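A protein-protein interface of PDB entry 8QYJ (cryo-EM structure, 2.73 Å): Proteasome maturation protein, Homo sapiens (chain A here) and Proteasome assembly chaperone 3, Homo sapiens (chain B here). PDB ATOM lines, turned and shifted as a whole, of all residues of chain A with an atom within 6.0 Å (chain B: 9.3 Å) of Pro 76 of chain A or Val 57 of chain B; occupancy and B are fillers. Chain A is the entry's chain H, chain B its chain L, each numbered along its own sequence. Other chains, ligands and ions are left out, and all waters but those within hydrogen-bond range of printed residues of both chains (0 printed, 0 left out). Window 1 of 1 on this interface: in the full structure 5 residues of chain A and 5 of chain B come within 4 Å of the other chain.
The side-chain carboxylate (OD1) of Asp 56 of chain B lies close to the backbone NH (N) of Ser 58 of chain B, 3.5 Å away. The backbone carbonyl oxygen of Ser 58 of chain B lies within hydrogen-bond range of the side-chain amide nitrogen of Asn 92 of chain B, at 3.1 Å.
Of the 13 printed residues of chain A, 4 touch a printed residue of chain B. Printed residues of chain A that touch a printed residue of chain B: Phe 64, Leu 73, Pro 76 and Gln 80. Hydrophobic or aromatic side chains of chain A that line the printed part of chain B: Phe 64, Leu 73 and Pro 76.
Of the printed residues of chain B, Gln 80 of chain A touches Val 57. Of the printed residues of chain A, Ser 55 of chain B touches Leu 73. Of the printed residues of chain A, Asp 56 of chain B touches Leu 73 (3.4 Å). Of the printed residues of chain B, Phe 64 of chain A touches Ser 58 (3.5 Å). Printed residues of chain B within 4 Å of Leu 73 of chain A: Ser 55 and Asp 56. Phe 74 of chain A touches none of the printed residues of chain B. Leu 79 of chain A touches none of the printed residues of chain B. The nearest residue of chain A that does not touch Val 57 of chain B is Leu 77 of chain A (4.1 Å).
Among the printed residues, pairs that only touch across the chains: Gln 80 of chain A with Val 57 of chain B (3.1 Å), Leu 73 of chain A with Asp 56 of chain B (3.4 Å), Phe 64 of chain A with Ser 58 of chain B (3.5 Å), Pro 76 of chain A with Val 57 of chain B (3.6 Å) and Leu 73 of chain A with Ser 55 of chain B (3.99 Å).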
ATOM      1  N   PHE A  64       7.142  21.468 -14.722  1.00  0.00           N
ATOM      2  CA  PHE A  64       8.331  20.800 -14.204  1.00  0.00           C
ATOM      3  C   PHE A  64       8.462  20.976 -12.696  1.00  0.00           C
ATOM      4  O   PHE A  64       8.857  20.042 -11.992  1.00  0.00           O
ATOM      5  CB  PHE A  64       9.580  21.322 -14.914  1.00  0.00           C
ATOM      6  CG  PHE A  64       9.908  20.587 -16.182  1.00  0.00           C
ATOM      7  CD1 PHE A  64       9.005  19.694 -16.735  1.00  0.00           C
ATOM      8  CD2 PHE A  64      11.120  20.787 -16.820  1.00  0.00           C
ATOM      9  CE1 PHE A  64       9.305  19.017 -17.902  1.00  0.00           C
ATOM     10  CE2 PHE A  64      11.425  20.113 -17.985  1.00  0.00           C
ATOM     11  CZ  PHE A  64      10.516  19.227 -18.526  1.00  0.00           C
ATOM     12  N   LEU A  67       5.972  18.664 -11.056  1.00  0.00           N
ATOM     13  CA  LEU A  67       6.429  17.285 -11.177  1.00  0.00           C
ATOM     14  C   LEU A  67       7.565  16.993 -10.205  1.00  0.00           C
ATOM     15  O   LEU A  67       7.599  15.925  -9.583  1.00  0.00           O
ATOM     16  CB  LEU A  67       6.863  17.005 -12.616  1.00  0.00           C
ATOM     17  CG  LEU A  67       7.131  15.549 -12.994  1.00  0.00           C
ATOM     18  CD1 LEU A  67       5.943  14.672 -12.644  1.00  0.00           C
ATOM     19  CD2 LEU A  67       7.460  15.442 -14.473  1.00  0.00           C
ATOM     20  N   ARG A  68       8.503  17.931 -10.059  1.00  0.00           N
ATOM     21  CA  ARG A  68       9.598  17.748  -9.114  1.00  0.00           C
ATOM     22  C   ARG A  68       9.088  17.694  -7.681  1.00  0.00           C
ATOM     23  O   ARG A  68       9.568  16.890  -6.872  1.00  0.00           O
ATOM     24  CB  ARG A  68      10.622  18.872  -9.276  1.00  0.00           C
ATOM     25  CG  ARG A  68      11.889  18.689  -8.455  1.00  0.00           C
ATOM     26  CD  ARG A  68      11.873  19.554  -7.205  1.00  0.00           C
ATOM     27  NE  ARG A  68      13.154  19.526  -6.507  1.00  0.00           N
ATOM     28  CZ  ARG A  68      13.490  18.628  -5.594  1.00  0.00           C
ATOM     29  NH1 ARG A  68      12.661  17.662  -5.235  1.00  0.00           N
ATOM     30  NH2 ARG A  68      14.689  18.700  -5.024  1.00  0.00           N
ATOM     31  N   GLY A  72       9.745  13.772  -7.767  1.00  0.00           N
ATOM     32  CA  GLY A  72      11.140  13.874  -7.398  1.00  0.00           C
ATOM     33  C   GLY A  72      11.950  14.495  -8.518  1.00  0.00           C
ATOM     34  O   GLY A  72      11.414  14.931  -9.532  1.00  0.00           O
ATOM     35  N   LEU A  73      13.267  14.520  -8.307  1.00  0.00           N
ATOM     36  CA  LEU A  73      14.179  15.151  -9.254  1.00  0.00           C
ATOM     37  C   LEU A  73      14.368  14.336 -10.527  1.00  0.00           C
ATOM     38  O   LEU A  73      14.841  14.880 -11.529  1.00  0.00           O
ATOM     39  CB  LEU A  73      15.539  15.383  -8.594  1.00  0.00           C
ATOM     40  CG  LEU A  73      15.732  16.675  -7.802  1.00  0.00           C
ATOM     41  CD1 LEU A  73      17.108  16.705  -7.160  1.00  0.00           C
ATOM     42  CD2 LEU A  73      15.530  17.886  -8.694  1.00  0.00           C
ATOM     43  N   PHE A  74      14.016  13.050 -10.510  1.00  0.00           N
ATOM     44  CA  PHE A  74      14.334  12.172 -11.632  1.00  0.00           C
ATOM     45  C   PHE A  74      13.418  12.382 -12.832  1.00  0.00           C
ATOM     46  O   PHE A  74      13.867  12.237 -13.973  1.00  0.00           O
ATOM     47  CB  PHE A  74      14.280  10.710 -11.183  1.00  0.00           C
ATOM     48  CG  PHE A  74      12.916  10.257 -10.744  1.00  0.00           C
ATOM     49  CD1 PHE A  74      12.484  10.470  -9.446  1.00  0.00           C
ATOM     50  CD2 PHE A  74      12.069   9.607 -11.627  1.00  0.00           C
ATOM     51  CE1 PHE A  74      11.234  10.054  -9.040  1.00  0.00           C
ATOM     52  CE2 PHE A  74      10.816   9.190 -11.225  1.00  0.00           C
ATOM     53  CZ  PHE A  74      10.399   9.413  -9.930  1.00  0.00           C
ATOM     54  N   ALA A  75      12.138  12.700 -12.604  1.00  0.00           N
ATOM     55  CA  ALA A  75      11.195  12.776 -13.720  1.00  0.00           C
ATOM     56  C   ALA A  75      11.520  13.899 -14.701  1.00  0.00           C
ATOM     57  O   ALA A  75      11.578  13.629 -15.916  1.00  0.00           O
ATOM     58  CB  ALA A  75       9.765  12.880 -13.183  1.00  0.00           C
ATOM     59  N   PRO A  76      11.715  15.156 -14.278  1.00  0.00           N
ATOM     60  CA  PRO A  76      12.093  16.187 -15.258  1.00  0.00           C
ATOM     61  C   PRO A  76      13.427  15.913 -15.924  1.00  0.00           C
ATOM     62  O   PRO A  76      13.606  16.248 -17.102  1.00  0.00           O
ATOM     63  CB  PRO A  76      12.126  17.476 -14.423  1.00  0.00           C
ATOM     64  CG  PRO A  76      11.368  17.164 -13.184  1.00  0.00           C
ATOM     65  CD  PRO A  76      11.618  15.723 -12.921  1.00  0.00           C
ATOM     66  N   LEU A  77      14.371  15.307 -15.201  1.00  0.00           N
ATOM     67  CA  LEU A  77      15.654  14.949 -15.794  1.00  0.00           C
ATOM     68  C   LEU A  77      15.472  13.934 -16.916  1.00  0.00           C
ATOM     69  O   LEU A  77      16.060  14.069 -17.996  1.00  0.00           O
ATOM     70  CB  LEU A  77      16.585  14.406 -14.710  1.00  0.00           C
ATOM     71  CG  LEU A  77      17.999  13.985 -15.108  1.00  0.00           C
ATOM     72  CD1 LEU A  77      18.952  15.163 -15.016  1.00  0.00           C
ATOM     73  CD2 LEU A  77      18.473  12.840 -14.231  1.00  0.00           C
ATOM     74  N   LYS A  78      14.642  12.914 -16.679  1.00  0.00           N
ATOM     75  CA  LYS A  78      14.353  11.929 -17.716  1.00  0.00           C
ATOM     76  C   LYS A  78      13.674  12.577 -18.913  1.00  0.00           C
ATOM     77  O   LYS A  78      14.014  12.282 -20.067  1.00  0.00           O
ATOM     78  CB  LYS A  78      13.475  10.814 -17.151  1.00  0.00           C
ATOM     79  CG  LYS A  78      14.229   9.667 -16.505  1.00  0.00           C
ATOM     80  CD  LYS A  78      13.258   8.646 -15.933  1.00  0.00           C
ATOM     81  CE  LYS A  78      13.986   7.507 -15.244  1.00  0.00           C
ATOM     82  NZ  LYS A  78      13.134   6.827 -14.232  1.00  0.00           N
ATOM     83  N   LEU A  79      12.708  13.463 -18.658  1.00  0.00           N
ATOM     84  CA  LEU A  79      12.014  14.128 -19.757  1.00  0.00           C
ATOM     85  C   LEU A  79      12.976  14.956 -20.601  1.00  0.00           C
ATOM     86  O   LEU A  79      12.931  14.909 -21.837  1.00  0.00           O
ATOM     87  CB  LEU A  79      10.887  15.006 -19.213  1.00  0.00           C
ATOM     88  CG  LEU A  79       9.702  14.284 -18.568  1.00  0.00           C
ATOM     89  CD1 LEU A  79       8.617  15.275 -18.185  1.00  0.00           C
ATOM     90  CD2 LEU A  79       9.151  13.221 -19.496  1.00  0.00           C
ATOM     91  N   GLN A  80      13.866  15.710 -19.952  1.00  0.00           N
ATOM     92  CA  GLN A  80      14.791  16.550 -20.705  1.00  0.00           C
ATOM     93  C   GLN A  80      15.818  15.717 -21.460  1.00  0.00           C
ATOM     94  O   GLN A  80      16.198  16.068 -22.584  1.00  0.00           O
ATOM     95  CB  GLN A  80      15.481  17.550 -19.779  1.00  0.00           C
ATOM     96  CG  GLN A  80      16.390  18.516 -20.519  1.00  0.00           C
ATOM     97  CD  GLN A  80      17.024  19.541 -19.609  1.00  0.00           C
ATOM     98  OE1 GLN A  80      16.820  19.520 -18.399  1.00  0.00           O
ATOM     99  NE2 GLN A  80      17.800  20.449 -20.189  1.00  0.00           N
ATOM    100  N   MET A  81      16.288  14.613 -20.869  1.00  0.00           N
ATOM    101  CA  MET A  81      17.209  13.749 -21.603  1.00  0.00           C
ATOM    102  C   MET A  81      16.536  13.135 -22.823  1.00  0.00           C
ATOM    103  O   MET A  81      17.151  13.038 -23.892  1.00  0.00           O
ATOM    104  CB  MET A  81      17.778  12.658 -20.698  1.00  0.00           C
ATOM    105  CG  MET A  81      18.683  13.173 -19.593  1.00  0.00           C
ATOM    106  SD  MET A  81      19.393  11.852 -18.592  1.00  0.00           S
ATOM    107  CE  MET A  81      17.977  11.348 -17.622  1.00  0.00           C
ATOM    108  N   PRO B  50      21.573  28.749 -18.413  1.00  0.00           N
ATOM    109  CA  PRO B  50      21.405  27.599 -17.517  1.00  0.00           C
ATOM    110  C   PRO B  50      22.368  26.479 -17.882  1.00  0.00           C
ATOM    111  O   PRO B  50      22.677  26.255 -19.053  1.00  0.00           O
ATOM    112  CB  PRO B  50      19.946  27.182 -17.740  1.00  0.00           C
ATOM    113  CG  PRO B  50      19.286  28.382 -18.336  1.00  0.00           C
ATOM    114  CD  PRO B  50      20.337  29.067 -19.146  1.00  0.00           C
ATOM    115  N   SER B  51      22.841  25.770 -16.861  1.00  0.00           N
ATOM    116  CA  SER B  51      23.768  24.670 -17.084  1.00  0.00           C
ATOM    117  C   SER B  51      23.052  23.488 -17.722  1.00  0.00           C
ATOM    118  O   SER B  51      21.896  23.194 -17.406  1.00  0.00           O
ATOM    119  CB  SER B  51      24.415  24.245 -15.768  1.00  0.00           C
ATOM    120  OG  SER B  51      25.474  23.332 -15.995  1.00  0.00           O
ATOM    121  N   SER B  52      23.747  22.807 -18.629  1.00  0.00           N
ATOM    122  CA  SER B  52      23.192  21.656 -19.329  1.00  0.00           C
ATOM    123  C   SER B  52      23.394  20.348 -18.578  1.00  0.00           C
ATOM    124  O   SER B  52      22.889  19.312 -19.023  1.00  0.00           O
ATOM    125  CB  SER B  52      23.807  21.545 -20.727  1.00  0.00           C
ATOM    126  OG  SER B  52      25.192  21.252 -20.653  1.00  0.00           O
ATOM    127  N   VAL B  53      24.114  20.365 -17.457  1.00  0.00           N
ATOM    128  CA  VAL B  53      24.367  19.154 -16.683  1.00  0.00           C
ATOM    129  C   VAL B  53      23.845  19.337 -15.265  1.00  0.00           C
ATOM    130  O   VAL B  53      24.340  18.708 -14.324  1.00  0.00           O
ATOM    131  CB  VAL B  53      25.865  18.799 -16.679  1.00  0.00           C
ATOM    132  CG1 VAL B  53      26.298  18.310 -18.050  1.00  0.00           C
ATOM    133  CG2 VAL B  53      26.692  20.000 -16.252  1.00  0.00           C
ATOM    134  N   ALA B  54      22.846  20.198 -15.104  1.00  0.00           N
ATOM    135  CA  ALA B  54      22.284  20.452 -13.786  1.00  0.00           C
ATOM    136  C   ALA B  54      21.403  19.292 -13.342  1.00  0.00           C
ATOM    137  O   ALA B  54      20.586  18.780 -14.112  1.00  0.00           O
ATOM    138  CB  ALA B  54      21.476  21.750 -13.794  1.00  0.00           C
ATOM    139  N   SER B  55      21.579  18.871 -12.087  1.00  0.00           N
ATOM    140  CA  SER B  55      20.746  17.802 -11.545  1.00  0.00           C
ATOM    141  C   SER B  55      19.330  18.294 -11.269  1.00  0.00           C
ATOM    142  O   SER B  55      18.359  17.560 -11.483  1.00  0.00           O
ATOM    143  CB  SER B  55      21.377  17.237 -10.273  1.00  0.00           C
ATOM    144  OG  SER B  55      21.706  18.271  -9.363  1.00  0.00           O
ATOM    145  N   ASP B  56      19.195  19.529 -10.790  1.00  0.00           N
ATOM    146  CA  ASP B  56      17.892  20.150 -10.554  1.00  0.00           C
ATOM    147  C   ASP B  56      17.592  21.035 -11.759  1.00  0.00           C
ATOM    148  O   ASP B  56      17.942  22.214 -11.792  1.00  0.00           O
ATOM    149  CB  ASP B  56      17.891  20.942  -9.251  1.00  0.00           C
ATOM    150  CG  ASP B  56      16.491  21.290  -8.780  1.00  0.00           C
ATOM    151  OD1 ASP B  56      15.537  21.145  -9.572  1.00  0.00           O
ATOM    152  OD2 ASP B  56      16.344  21.711  -7.614  1.00  0.00           O
ATOM    153  N   VAL B  57      16.930  20.452 -12.761  1.00  0.00           N
ATOM    154  CA  VAL B  57      16.667  21.167 -14.007  1.00  0.00           C
ATOM    155  C   VAL B  57      15.536  22.172 -13.886  1.00  0.00           C
ATOM    156  O   VAL B  57      15.372  23.013 -14.779  1.00  0.00           O
ATOM    157  CB  VAL B  57      16.359  20.169 -15.136  1.00  0.00           C
ATOM    158  CG1 VAL B  57      17.556  19.265 -15.375  1.00  0.00           C
ATOM    159  CG2 VAL B  57      15.132  19.352 -14.798  1.00  0.00           C
ATOM    160  N   SER B  58      14.744  22.108 -12.813  1.00  0.00           N
ATOM    161  CA  SER B  58      13.714  23.119 -12.597  1.00  0.00           C
ATOM    162  C   SER B  58      14.327  24.436 -12.139  1.00  0.00           C
ATOM    163  O   SER B  58      13.872  25.513 -12.541  1.00  0.00           O
ATOM    164  CB  SER B  58      12.693  22.618 -11.577  1.00  0.00           C
ATOM    165  OG  SER B  58      12.103  21.403 -12.004  1.00  0.00           O
ATOM    166  N   LYS B  59      15.357  24.369 -11.298  1.00  0.00           N
ATOM    167  CA  LYS B  59      16.090  25.544 -10.828  1.00  0.00           C
ATOM    168  C   LYS B  59      17.577  25.303 -11.046  1.00  0.00           C
ATOM    169  O   LYS B  59      18.326  25.039 -10.098  1.00  0.00           O
ATOM    170  CB  LYS B  59      15.786  25.831  -9.357  1.00  0.00           C
ATOM    171  CG  LYS B  59      14.349  26.241  -9.091  1.00  0.00           C
ATOM    172  CD  LYS B  59      14.118  26.525  -7.617  1.00  0.00           C
ATOM    173  CE  LYS B  59      12.703  27.023  -7.368  1.00  0.00           C
ATOM    174  NZ  LYS B  59      11.689  25.968  -7.642  1.00  0.00           N
ATOM    175  N   PRO B  60      18.038  25.382 -12.289  1.00  0.00           N
ATOM    176  CA  PRO B  60      19.432  25.051 -12.587  1.00  0.00           C
ATOM    177  C   PRO B  60      20.387  26.164 -12.185  1.00  0.00           C
ATOM    178  O   PRO B  60      19.996  27.304 -11.926  1.00  0.00           O
ATOM    179  CB  PRO B  60      19.426  24.857 -14.106  1.00  0.00           C
ATOM    180  CG  PRO B  60      18.344  25.761 -14.583  1.00  0.00           C
ATOM    181  CD  PRO B  60      17.308  25.832 -13.488  1.00  0.00           C
ATOM    182  N   VAL B  61      21.669  25.803 -12.132  1.00  0.00           N
ATOM    183  CA  VAL B  61      22.713  26.780 -11.859  1.00  0.00           C
ATOM    184  C   VAL B  61      23.082  27.512 -13.144  1.00  0.00           C
ATOM    185  O   VAL B  61      22.900  27.011 -14.257  1.00  0.00           O
ATOM    186  CB  VAL B  61      23.944  26.111 -11.221  1.00  0.00           C
ATOM    187  CG1 VAL B  61      23.581  25.516  -9.871  1.00  0.00           C
ATOM    188  CG2 VAL B  61      24.505  25.044 -12.144  1.00  0.00           C
ATOM    189  N   GLY B  91      11.295  31.961 -16.911  1.00  0.00           N
ATOM    190  CA  GLY B  91      11.108  30.594 -17.349  1.00  0.00           C
ATOM    191  C   GLY B  91      12.413  29.901 -17.678  1.00  0.00           C
ATOM    192  O   GLY B  91      12.481  29.112 -18.625  1.00  0.00           O
ATOM    193  N   ASN B  92      13.452  30.192 -16.894  1.00  0.00           N
ATOM    194  CA  ASN B  92      14.789  29.629 -17.097  1.00  0.00           C
ATOM    195  C   ASN B  92      15.309  29.940 -18.499  1.00  0.00           C
ATOM    196  O   ASN B  92      15.723  29.053 -19.247  1.00  0.00           O
ATOM    197  CB  ASN B  92      14.800  28.123 -16.824  1.00  0.00           C
ATOM    198  CG  ASN B  92      14.439  27.789 -15.390  1.00  0.00           C
ATOM    199  OD1 ASN B  92      15.118  28.207 -14.454  1.00  0.00           O
ATOM    200  ND2 ASN B  92      13.364  27.031 -15.213  1.00  0.00           N
ATOM    201  N   ARG B  93      15.283  31.221 -18.851  1.00  0.00           N
ATOM    202  CA  ARG B  93      15.743  31.696 -20.146  1.00  0.00           C
ATOM    203  C   ARG B  93      17.093  32.388 -19.997  1.00  0.00           C
ATOM    204  O   ARG B  93      17.406  32.954 -18.946  1.00  0.00           O
ATOM    205  CB  ARG B  93      14.729  32.659 -20.770  1.00  0.00           C
ATOM    206  CG  ARG B  93      14.659  32.586 -22.283  1.00  0.00           C
ATOM    207  CD  ARG B  93      13.672  33.592 -22.850  1.00  0.00           C
ATOM    208  NE  ARG B  93      12.313  33.357 -22.380  1.00  0.00           N
ATOM    209  CZ  ARG B  93      11.393  34.303 -22.243  1.00  0.00           C
ATOM    210  NH1 ARG B  93      11.649  35.564 -22.549  1.00  0.00           N
ATOM    211  NH2 ARG B  93      10.186  33.974 -21.794  1.00  0.00           N
